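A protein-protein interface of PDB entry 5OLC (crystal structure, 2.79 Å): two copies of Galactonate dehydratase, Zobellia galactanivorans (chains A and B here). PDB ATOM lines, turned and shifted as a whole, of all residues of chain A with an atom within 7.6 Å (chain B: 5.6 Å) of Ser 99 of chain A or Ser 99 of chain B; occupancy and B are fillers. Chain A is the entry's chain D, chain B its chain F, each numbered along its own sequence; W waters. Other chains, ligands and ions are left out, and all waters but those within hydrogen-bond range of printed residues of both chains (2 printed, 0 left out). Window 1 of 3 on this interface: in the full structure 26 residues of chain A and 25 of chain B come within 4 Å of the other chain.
NH2 of Arg 98 of chain A lies within salt-bridge range of OE2 of Glu 256 of chain B (2.8 Å). The backbone carbonyl oxygen (O) of Ala 97 of chain A sits at hydrogen-bond distance from the backbone NH (N) of Gly 100 of chain B (3.0 Å). The guanidinium group of Arg 98 of chain B is in salt-bridge range of the side-chain carboxylate of Glu 256 of chain A, at 3.1 Å. The guanidinium group (NH2) of Arg 98 of chain A lies within hydrogen-bond range of the backbone carbonyl oxygen (O) of Cys 255 of chain B (3.2 Å). The backbone carbonyl oxygen (O) of Ala 97 of chain B is in hydrogen-bond range of the backbone NH (N) of Gly 100 of chain A, at 3.4 Å. NH2 of Arg 98 of chain B is in hydrogen-bond range of O of Cys 255 of chain A (3.2 Å). OE2 of Glu 234 of chain A lies within salt-bridge range of NH1 of Arg 98 of chain B (2.8 Å).
The side-chain amide oxygen of Gln 103 of chain B sits at hydrogen-bond distance from the backbone NH of Arg 98 of chain B, at 2.8 Å.
Among the printed residues, pairs that only touch across the chains: Tyr 96 of chain A with Gly 100 of chain B, Tyr 96 of chain A with Val 101 of chain B, Tyr 96 of chain A with Tyr 257 of chain B, Ala 97 of chain A with Ser 99 of chain B, Arg 98 of chain A with Ser 99 of chain B, Ser 99 of chain A with Ala 97 of chain B, Ser 99 of chain A with Ser 99 of chain B, Val 101 of chain A with Val 101 of chain B, Val 101 of chain A with Leu 102 of chain B and Leu 102 of chain A with Val 101 of chain B.
Of chain B, only Ala 97 and Ser 99 come within 4 Å of Ser 99 of chain A. Of the printed residues of chain B, Val 101 of chain A touches Val 101 (3.9 Å) and Leu 102 (3.8 Å). Of the printed residues of chain B, Leu 102 of chain A touches Val 101 (3.8 Å). Printed residues of chain B within 4 Å of Glu 234 of chain A: Arg 98. Leu 258 of chain A touches none of the printed residues of chain B. Ala 280 of chain A touches none of the printed residues of chain B. Of chain A, only Ala 97 (3.3 Å), Arg 98 (3.8 Å) and Ser 99 (3.6 Å) come within 4 Å of Ser 99 of chain B. Printed residues of chain A within 4 Å of Leu 102 of chain B: Val 101 (3.8 Å). Of the printed residues of chain A, Tyr 257 of chain B touches Tyr 96 (3.9 Å). The nearest residue of chain B that does not touch Ser 99 of chain A is Arg 98 of chain B (4.2 Å). The nearest residue of chain A that does not touch Ser 99 of chain B is Gly 100 of chain A (4.4 Å). The nearest printed residue of chain A that does not touch Glu 256 of chain B is Ala 97 of chain A (8.0 Å).
Hydrophobic or aromatic side chains of chain B that line the printed part of chain A: Val 101, Leu 102 and Tyr 257. Printed residues of chain A that touch a printed residue of chain B: Tyr 96, Ala 97, Arg 98, Ser 99, Gly 100, Val 101, Leu 102, Glu 234, Cys 255 and Glu 256. Along chain A the printed residues that touch a printed residue of chain B span positions 96 to 256. Among the printed residues, Asp or Glu carboxylates within 4 Å of a Lys or Arg side-chain nitrogen of the other chain: Arg 98 of chain A with Glu 256 of chain B (2.8 Å), Glu 234 of chain A with Arg 98 of chain B (2.8 Å) and Glu 256 of chain A with Arg 98 of chain B (3.1 Å).
Ala 97 of chain A touches Ser 99 of chain B, and with the chains exchanged Ser 99 of chain A touches Ala 97 of chain B. Ala 97 of chain A touches Gly 100 of chain B, and with the chains exchanged Gly 100 of chain A touches Ala 97 of chain B. Val 101 of chain B touches its own counterpart, Val 101 of chain A. Val 101 of chain A touches Leu 102 of chain B, and with the chains exchanged Leu 102 of chain A touches Val 101 of chain B.
Water W1 lies within hydrogen-bond range of O of Ser 99 of chain A, N of Val 101 of chain B and N of Leu 102 of chain A. Water W2 lies within hydrogen-bond range of NE of Arg 98 of chain A (3.4 Å) and OG of Ser 99 of chain B (3.4 Å).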
ATOM      1  N   SER A  93       0.594  14.635  13.906  1.00  0.00           N
ATOM      2  CA  SER A  93      -0.224  15.838  13.657  1.00  0.00           C
ATOM      3  C   SER A  93      -0.348  16.336  12.175  1.00  0.00           C
ATOM      4  O   SER A  93      -1.101  17.279  11.941  1.00  0.00           O
ATOM      5  CB  SER A  93       0.269  16.993  14.532  1.00  0.00           C
ATOM      6  OG  SER A  93       1.326  17.744  13.948  1.00  0.00           O
ATOM      7  N   TYR A  96      -3.927  16.890  11.011  1.00  0.00           N
ATOM      8  CA  TYR A  96      -4.708  17.865  11.799  1.00  0.00           C
ATOM      9  C   TYR A  96      -3.928  19.142  12.215  1.00  0.00           C
ATOM     10  O   TYR A  96      -4.347  19.843  13.144  1.00  0.00           O
ATOM     11  CB  TYR A  96      -5.301  17.191  13.065  1.00  0.00           C
ATOM     12  CG  TYR A  96      -5.621  15.721  12.925  1.00  0.00           C
ATOM     13  CD1 TYR A  96      -6.759  15.298  12.243  1.00  0.00           C
ATOM     14  CD2 TYR A  96      -4.818  14.755  13.520  1.00  0.00           C
ATOM     15  CE1 TYR A  96      -7.076  13.945  12.133  1.00  0.00           C
ATOM     16  CE2 TYR A  96      -5.128  13.397  13.421  1.00  0.00           C
ATOM     17  CZ  TYR A  96      -6.258  12.997  12.721  1.00  0.00           C
ATOM     18  OH  TYR A  96      -6.584  11.667  12.589  1.00  0.00           O
ATOM     19  N   ALA A  97      -2.802  19.436  11.557  1.00  0.00           N
ATOM     20  CA  ALA A  97      -2.005  20.606  11.925  1.00  0.00           C
ATOM     21  C   ALA A  97      -1.688  21.494  10.725  1.00  0.00           C
ATOM     22  O   ALA A  97      -2.582  22.237  10.306  1.00  0.00           O
ATOM     23  CB  ALA A  97      -0.740  20.193  12.661  1.00  0.00           C
ATOM     24  N   ARG A  98      -0.438  21.417  10.160  1.00  0.00           N
ATOM     25  CA  ARG A  98       0.054  22.216   9.018  1.00  0.00           C
ATOM     26  C   ARG A  98       0.399  23.653   9.432  1.00  0.00           C
ATOM     27  O   ARG A  98       1.456  24.170   9.054  1.00  0.00           O
ATOM     28  CB  ARG A  98      -0.918  22.201   7.820  1.00  0.00           C
ATOM     29  CG  ARG A  98      -1.158  20.819   7.216  1.00  0.00           C
ATOM     30  CD  ARG A  98      -1.921  20.924   5.916  1.00  0.00           C
ATOM     31  NE  ARG A  98      -1.108  21.531   4.868  1.00  0.00           N
ATOM     32  CZ  ARG A  98      -1.521  21.733   3.626  1.00  0.00           C
ATOM     33  NH1 ARG A  98      -0.703  22.272   2.727  1.00  0.00           N
ATOM     34  NH2 ARG A  98      -2.754  21.385   3.265  1.00  0.00           N
ATOM     35  N   SER A  99      -0.487  24.282  10.217  1.00  0.00           N
ATOM     36  CA  SER A  99      -0.316  25.617  10.769  1.00  0.00           C
ATOM     37  C   SER A  99      -0.886  25.679  12.199  1.00  0.00           C
ATOM     38  O   SER A  99      -1.362  24.672  12.744  1.00  0.00           O
ATOM     39  CB  SER A  99      -0.987  26.658   9.878  1.00  0.00           C
ATOM     40  OG  SER A  99      -0.082  27.253   8.965  1.00  0.00           O
ATOM     41  N   GLY A 100      -0.767  26.864  12.788  1.00  0.00           N
ATOM     42  CA  GLY A 100      -1.294  27.235  14.090  1.00  0.00           C
ATOM     43  C   GLY A 100      -0.833  26.504  15.331  1.00  0.00           C
ATOM     44  O   GLY A 100       0.361  26.297  15.552  1.00  0.00           O
ATOM     45  N   VAL A 101      -1.836  26.176  16.173  1.00  0.00           N
ATOM     46  CA  VAL A 101      -1.811  25.586  17.509  1.00  0.00           C
ATOM     47  C   VAL A 101      -0.906  24.340  17.633  1.00  0.00           C
ATOM     48  O   VAL A 101       0.037  24.417  18.418  1.00  0.00           O
ATOM     49  CB  VAL A 101      -3.265  25.334  18.017  1.00  0.00           C
ATOM     50  CG1 VAL A 101      -3.310  24.376  19.210  1.00  0.00           C
ATOM     51  CG2 VAL A 101      -3.946  26.649  18.373  1.00  0.00           C
ATOM     52  N   LEU A 102      -1.161  23.217  16.912  1.00  0.00           N
ATOM     53  CA  LEU A 102      -0.301  22.029  17.066  1.00  0.00           C
ATOM     54  C   LEU A 102       1.171  22.290  16.677  1.00  0.00           C
ATOM     55  O   LEU A 102       2.053  21.606  17.195  1.00  0.00           O
ATOM     56  CB  LEU A 102      -0.850  20.782  16.370  1.00  0.00           C
ATOM     57  CG  LEU A 102      -2.000  20.058  17.076  1.00  0.00           C
ATOM     58  CD1 LEU A 102      -2.631  19.029  16.166  1.00  0.00           C
ATOM     59  CD2 LEU A 102      -1.549  19.362  18.345  1.00  0.00           C
ATOM     60  N   GLN A 103       1.438  23.321  15.835  1.00  0.00           N
ATOM     61  CA  GLN A 103       2.798  23.717  15.461  1.00  0.00           C
ATOM     62  C   GLN A 103       3.501  24.395  16.626  1.00  0.00           C
ATOM     63  O   GLN A 103       4.699  24.153  16.835  1.00  0.00           O
ATOM     64  CB  GLN A 103       2.857  24.582  14.177  1.00  0.00           C
ATOM     65  CG  GLN A 103       2.536  23.840  12.877  1.00  0.00           C
ATOM     66  CD  GLN A 103       3.077  22.421  12.817  1.00  0.00           C
ATOM     67  OE1 GLN A 103       4.281  22.167  12.983  1.00  0.00           O
ATOM     68  NE2 GLN A 103       2.187  21.458  12.610  1.00  0.00           N
ATOM     69  N   ALA A 104       2.745  25.197  17.414  1.00  0.00           N
ATOM     70  CA  ALA A 104       3.275  25.866  18.599  1.00  0.00           C
ATOM     71  C   ALA A 104       3.486  24.847  19.756  1.00  0.00           C
ATOM     72  O   ALA A 104       4.353  25.057  20.611  1.00  0.00           O
ATOM     73  CB  ALA A 104       2.370  27.013  19.017  1.00  0.00           C
ATOM     74  N   GLU A 234      -2.474  35.987   3.991  1.00  0.00           N
ATOM     75  CA  GLU A 234      -3.162  35.270   2.938  1.00  0.00           C
ATOM     76  C   GLU A 234      -3.072  36.010   1.588  1.00  0.00           C
ATOM     77  O   GLU A 234      -3.194  35.378   0.539  1.00  0.00           O
ATOM     78  CB  GLU A 234      -4.617  35.114   3.364  1.00  0.00           C
ATOM     79  CG  GLU A 234      -5.109  33.695   3.251  1.00  0.00           C
ATOM     80  CD  GLU A 234      -4.626  32.621   4.206  1.00  0.00           C
ATOM     81  OE1 GLU A 234      -5.074  32.615   5.376  1.00  0.00           O
ATOM     82  OE2 GLU A 234      -3.936  31.689   3.728  1.00  0.00           O
ATOM     83  N   CYS A 255       2.806  34.763  10.797  1.00  0.00           N
ATOM     84  CA  CYS A 255       1.717  33.801  10.622  1.00  0.00           C
ATOM     85  C   CYS A 255       2.049  32.637   9.663  1.00  0.00           C
ATOM     86  O   CYS A 255       1.154  31.856   9.314  1.00  0.00           O
ATOM     87  CB  CYS A 255       0.448  34.536  10.201  1.00  0.00           C
ATOM     88  SG  CYS A 255       0.153  36.072  11.117  1.00  0.00           S
ATOM     89  N   GLU A 256       3.335  32.502   9.265  1.00  0.00           N
ATOM     90  CA  GLU A 256       3.777  31.405   8.396  1.00  0.00           C
ATOM     91  C   GLU A 256       4.380  30.272   9.211  1.00  0.00           C
ATOM     92  O   GLU A 256       5.145  30.518  10.143  1.00  0.00           O
ATOM     93  CB  GLU A 256       4.711  31.898   7.284  1.00  0.00           C
ATOM     94  CG  GLU A 256       3.995  32.502   6.088  1.00  0.00           C
ATOM     95  CD  GLU A 256       3.188  31.552   5.225  1.00  0.00           C
ATOM     96  OE1 GLU A 256       3.436  30.327   5.275  1.00  0.00           O
ATOM     97  OE2 GLU A 256       2.306  32.044   4.486  1.00  0.00           O
ATOM     98  N   TYR A 257       3.978  29.037   8.892  1.00  0.00           N
ATOM     99  CA  TYR A 257       4.372  27.831   9.615  1.00  0.00           C
ATOM    100  C   TYR A 257       4.998  26.793   8.701  1.00  0.00           C
ATOM    101  O   TYR A 257       4.493  26.547   7.608  1.00  0.00           O
ATOM    102  CB  TYR A 257       3.152  27.221  10.344  1.00  0.00           C
ATOM    103  CG  TYR A 257       2.510  28.132  11.379  1.00  0.00           C
ATOM    104  CD1 TYR A 257       1.590  29.112  11.004  1.00  0.00           C
ATOM    105  CD2 TYR A 257       2.786  27.985  12.735  1.00  0.00           C
ATOM    106  CE1 TYR A 257       1.014  29.966  11.948  1.00  0.00           C
ATOM    107  CE2 TYR A 257       2.206  28.825  13.690  1.00  0.00           C
ATOM    108  CZ  TYR A 257       1.323  29.816  13.292  1.00  0.00           C
ATOM    109  OH  TYR A 257       0.744  30.629  14.237  1.00  0.00           O
ATOM    110  N   LEU A 258       6.087  26.163   9.171  1.00  0.00           N
ATOM    111  CA  LEU A 258       6.871  25.093   8.530  1.00  0.00           C
ATOM    112  C   LEU A 258       7.677  25.545   7.318  1.00  0.00           C
ATOM    113  O   LEU A 258       7.516  26.666   6.812  1.00  0.00           O
ATOM    114  CB  LEU A 258       6.018  23.848   8.173  1.00  0.00           C
ATOM    115  CG  LEU A 258       5.220  23.182   9.307  1.00  0.00           C
ATOM    116  CD1 LEU A 258       4.497  21.965   8.801  1.00  0.00           C
ATOM    117  CD2 LEU A 258       6.116  22.769  10.478  1.00  0.00           C
ATOM    118  N   GLY A 261       5.444  26.164   4.265  1.00  0.00           N
ATOM    119  CA  GLY A 261       4.796  27.461   4.323  1.00  0.00           C
ATOM    120  C   GLY A 261       5.724  28.564   3.863  1.00  0.00           C
ATOM    121  O   GLY A 261       5.315  29.431   3.092  1.00  0.00           O
ATOM    122  N   ALA A 280       6.481  29.163  17.236  1.00  0.00           N
ATOM    123  CA  ALA A 280       5.255  28.932  16.476  1.00  0.00           C
ATOM    124  C   ALA A 280       5.466  28.098  15.202  1.00  0.00           C
ATOM    125  O   ALA A 280       4.741  27.124  15.007  1.00  0.00           O
ATOM    126  CB  ALA A 280       4.606  30.265  16.135  1.00  0.00           C
ATOM    127  N   ALA B  97      -4.030  30.643  13.602  1.00  0.00           N
ATOM    128  CA  ALA B  97      -4.779  29.515  13.061  1.00  0.00           C
ATOM    129  C   ALA B  97      -4.384  29.184  11.631  1.00  0.00           C
ATOM    130  O   ALA B  97      -3.313  28.596  11.447  1.00  0.00           O
ATOM    131  CB  ALA B  97      -6.276  29.746  13.189  1.00  0.00           C
ATOM    132  N   ARG B  98      -5.222  29.558  10.622  1.00  0.00           N
ATOM    133  CA  ARG B  98      -5.030  29.279   9.182  1.00  0.00           C
ATOM    134  C   ARG B  98      -5.344  27.811   8.837  1.00  0.00           C
ATOM    135  O   ARG B  98      -6.249  27.540   8.057  1.00  0.00           O
ATOM    136  CB  ARG B  98      -3.647  29.723   8.647  1.00  0.00           C
ATOM    137  CG  ARG B  98      -3.383  31.215   8.808  1.00  0.00           C
ATOM    138  CD  ARG B  98      -2.070  31.627   8.178  1.00  0.00           C
ATOM    139  NE  ARG B  98      -2.135  31.587   6.720  1.00  0.00           N
ATOM    140  CZ  ARG B  98      -1.190  32.066   5.922  1.00  0.00           C
ATOM    141  NH1 ARG B  98      -1.335  32.015   4.607  1.00  0.00           N
ATOM    142  NH2 ARG B  98      -0.095  32.609   6.433  1.00  0.00           N
ATOM    143  N   SER B  99      -4.611  26.872   9.429  1.00  0.00           N
ATOM    144  CA  SER B  99      -4.830  25.437   9.259  1.00  0.00           C
ATOM    145  C   SER B  99      -4.928  24.846  10.674  1.00  0.00           C
ATOM    146  O   SER B  99      -4.767  25.580  11.657  1.00  0.00           O
ATOM    147  CB  SER B  99      -3.674  24.797   8.486  1.00  0.00           C
ATOM    148  OG  SER B  99      -4.048  24.234   7.238  1.00  0.00           O
ATOM    149  N   GLY B 100      -5.245  23.555  10.761  1.00  0.00           N
ATOM    150  CA  GLY B 100      -5.322  22.827  12.022  1.00  0.00           C
ATOM    151  C   GLY B 100      -6.480  23.067  12.970  1.00  0.00           C
ATOM    152  O   GLY B 100      -7.599  23.393  12.562  1.00  0.00           O
ATOM    153  N   VAL B 101      -6.166  22.897  14.271  1.00  0.00           N
ATOM    154  CA  VAL B 101      -6.996  22.889  15.482  1.00  0.00           C
ATOM    155  C   VAL B 101      -8.017  24.064  15.606  1.00  0.00           C
ATOM    156  O   VAL B 101      -9.209  23.762  15.737  1.00  0.00           O
ATOM    157  CB  VAL B 101      -6.074  22.755  16.739  1.00  0.00           C
ATOM    158  CG1 VAL B 101      -6.775  23.167  18.037  1.00  0.00           C
ATOM    159  CG2 VAL B 101      -5.534  21.330  16.855  1.00  0.00           C
ATOM    160  N   LEU B 102      -7.590  25.357  15.594  1.00  0.00           N
ATOM    161  CA  LEU B 102      -8.566  26.451  15.774  1.00  0.00           C
ATOM    162  C   LEU B 102      -9.652  26.507  14.673  1.00  0.00           C
ATOM    163  O   LEU B 102     -10.735  27.037  14.918  1.00  0.00           O
ATOM    164  CB  LEU B 102      -7.907  27.819  15.964  1.00  0.00           C
ATOM    165  CG  LEU B 102      -7.337  28.124  17.335  1.00  0.00           C
ATOM    166  CD1 LEU B 102      -6.494  29.352  17.295  1.00  0.00           C
ATOM    167  CD2 LEU B 102      -8.421  28.329  18.365  1.00  0.00           C
ATOM    168  N   GLN B 103      -9.379  25.932  13.489  1.00  0.00           N
ATOM    169  CA  GLN B 103     -10.363  25.866  12.417  1.00  0.00           C
ATOM    170  C   GLN B 103     -11.424  24.818  12.765  1.00  0.00           C
ATOM    171  O   GLN B 103     -12.603  25.019  12.457  1.00  0.00           O
ATOM    172  CB  GLN B 103      -9.709  25.582  11.053  1.00  0.00           C
ATOM    173  CG  GLN B 103      -8.506  26.472  10.697  1.00  0.00           C
ATOM    174  CD  GLN B 103      -8.766  27.968  10.740  1.00  0.00           C
ATOM    175  OE1 GLN B 103      -7.871  28.759  11.049  1.00  0.00           O
ATOM    176  NE2 GLN B 103      -9.983  28.398  10.403  1.00  0.00           N
ATOM    177  N   CYS B 255      -6.948  17.482   4.600  1.00  0.00           N
ATOM    178  CA  CYS B 255      -5.996  18.368   5.283  1.00  0.00           C
ATOM    179  C   CYS B 255      -5.993  19.824   4.767  1.00  0.00           C
ATOM    180  O   CYS B 255      -5.144  20.631   5.178  1.00  0.00           O
ATOM    181  CB  CYS B 255      -4.594  17.765   5.246  1.00  0.00           C
ATOM    182  SG  CYS B 255      -4.542  15.980   5.527  1.00  0.00           S
ATOM    183  N   GLU B 256      -6.949  20.165   3.898  1.00  0.00           N
ATOM    184  CA  GLU B 256      -7.057  21.515   3.364  1.00  0.00           C
ATOM    185  C   GLU B 256      -8.078  22.315   4.141  1.00  0.00           C
ATOM    186  O   GLU B 256      -9.169  21.812   4.420  1.00  0.00           O
ATOM    187  CB  GLU B 256      -7.318  21.499   1.857  1.00  0.00           C
ATOM    188  CG  GLU B 256      -6.071  21.256   1.026  1.00  0.00           C
ATOM    189  CD  GLU B 256      -5.051  22.379   1.057  1.00  0.00           C
ATOM    190  OE1 GLU B 256      -5.446  23.548   1.284  1.00  0.00           O
ATOM    191  OE2 GLU B 256      -3.853  22.085   0.840  1.00  0.00           O
ATOM    192  N   TYR B 257      -7.666  23.528   4.581  1.00  0.00           N
ATOM    193  CA  TYR B 257      -8.435  24.445   5.442  1.00  0.00           C
ATOM    194  C   TYR B 257      -8.705  25.790   4.797  1.00  0.00           C
ATOM    195  O   TYR B 257      -7.813  26.370   4.198  1.00  0.00           O
ATOM    196  CB  TYR B 257      -7.727  24.647   6.815  1.00  0.00           C
ATOM    197  CG  TYR B 257      -7.629  23.380   7.635  1.00  0.00           C
ATOM    198  CD1 TYR B 257      -6.675  22.407   7.344  1.00  0.00           C
ATOM    199  CD2 TYR B 257      -8.504  23.140   8.683  1.00  0.00           C
ATOM    200  CE1 TYR B 257      -6.601  21.220   8.072  1.00  0.00           C
ATOM    201  CE2 TYR B 257      -8.440  21.958   9.423  1.00  0.00           C
ATOM    202  CZ  TYR B 257      -7.484  21.001   9.116  1.00  0.00           C
ATOM    203  OH  TYR B 257      -7.400  19.850   9.860  1.00  0.00           O
HETATM  204  O   HOH W   1      -3.068  23.291  14.424  1.00  0.00           O
HETATM  205  O   HOH W   2      -1.489  24.867   5.122  1.00  0.00           O
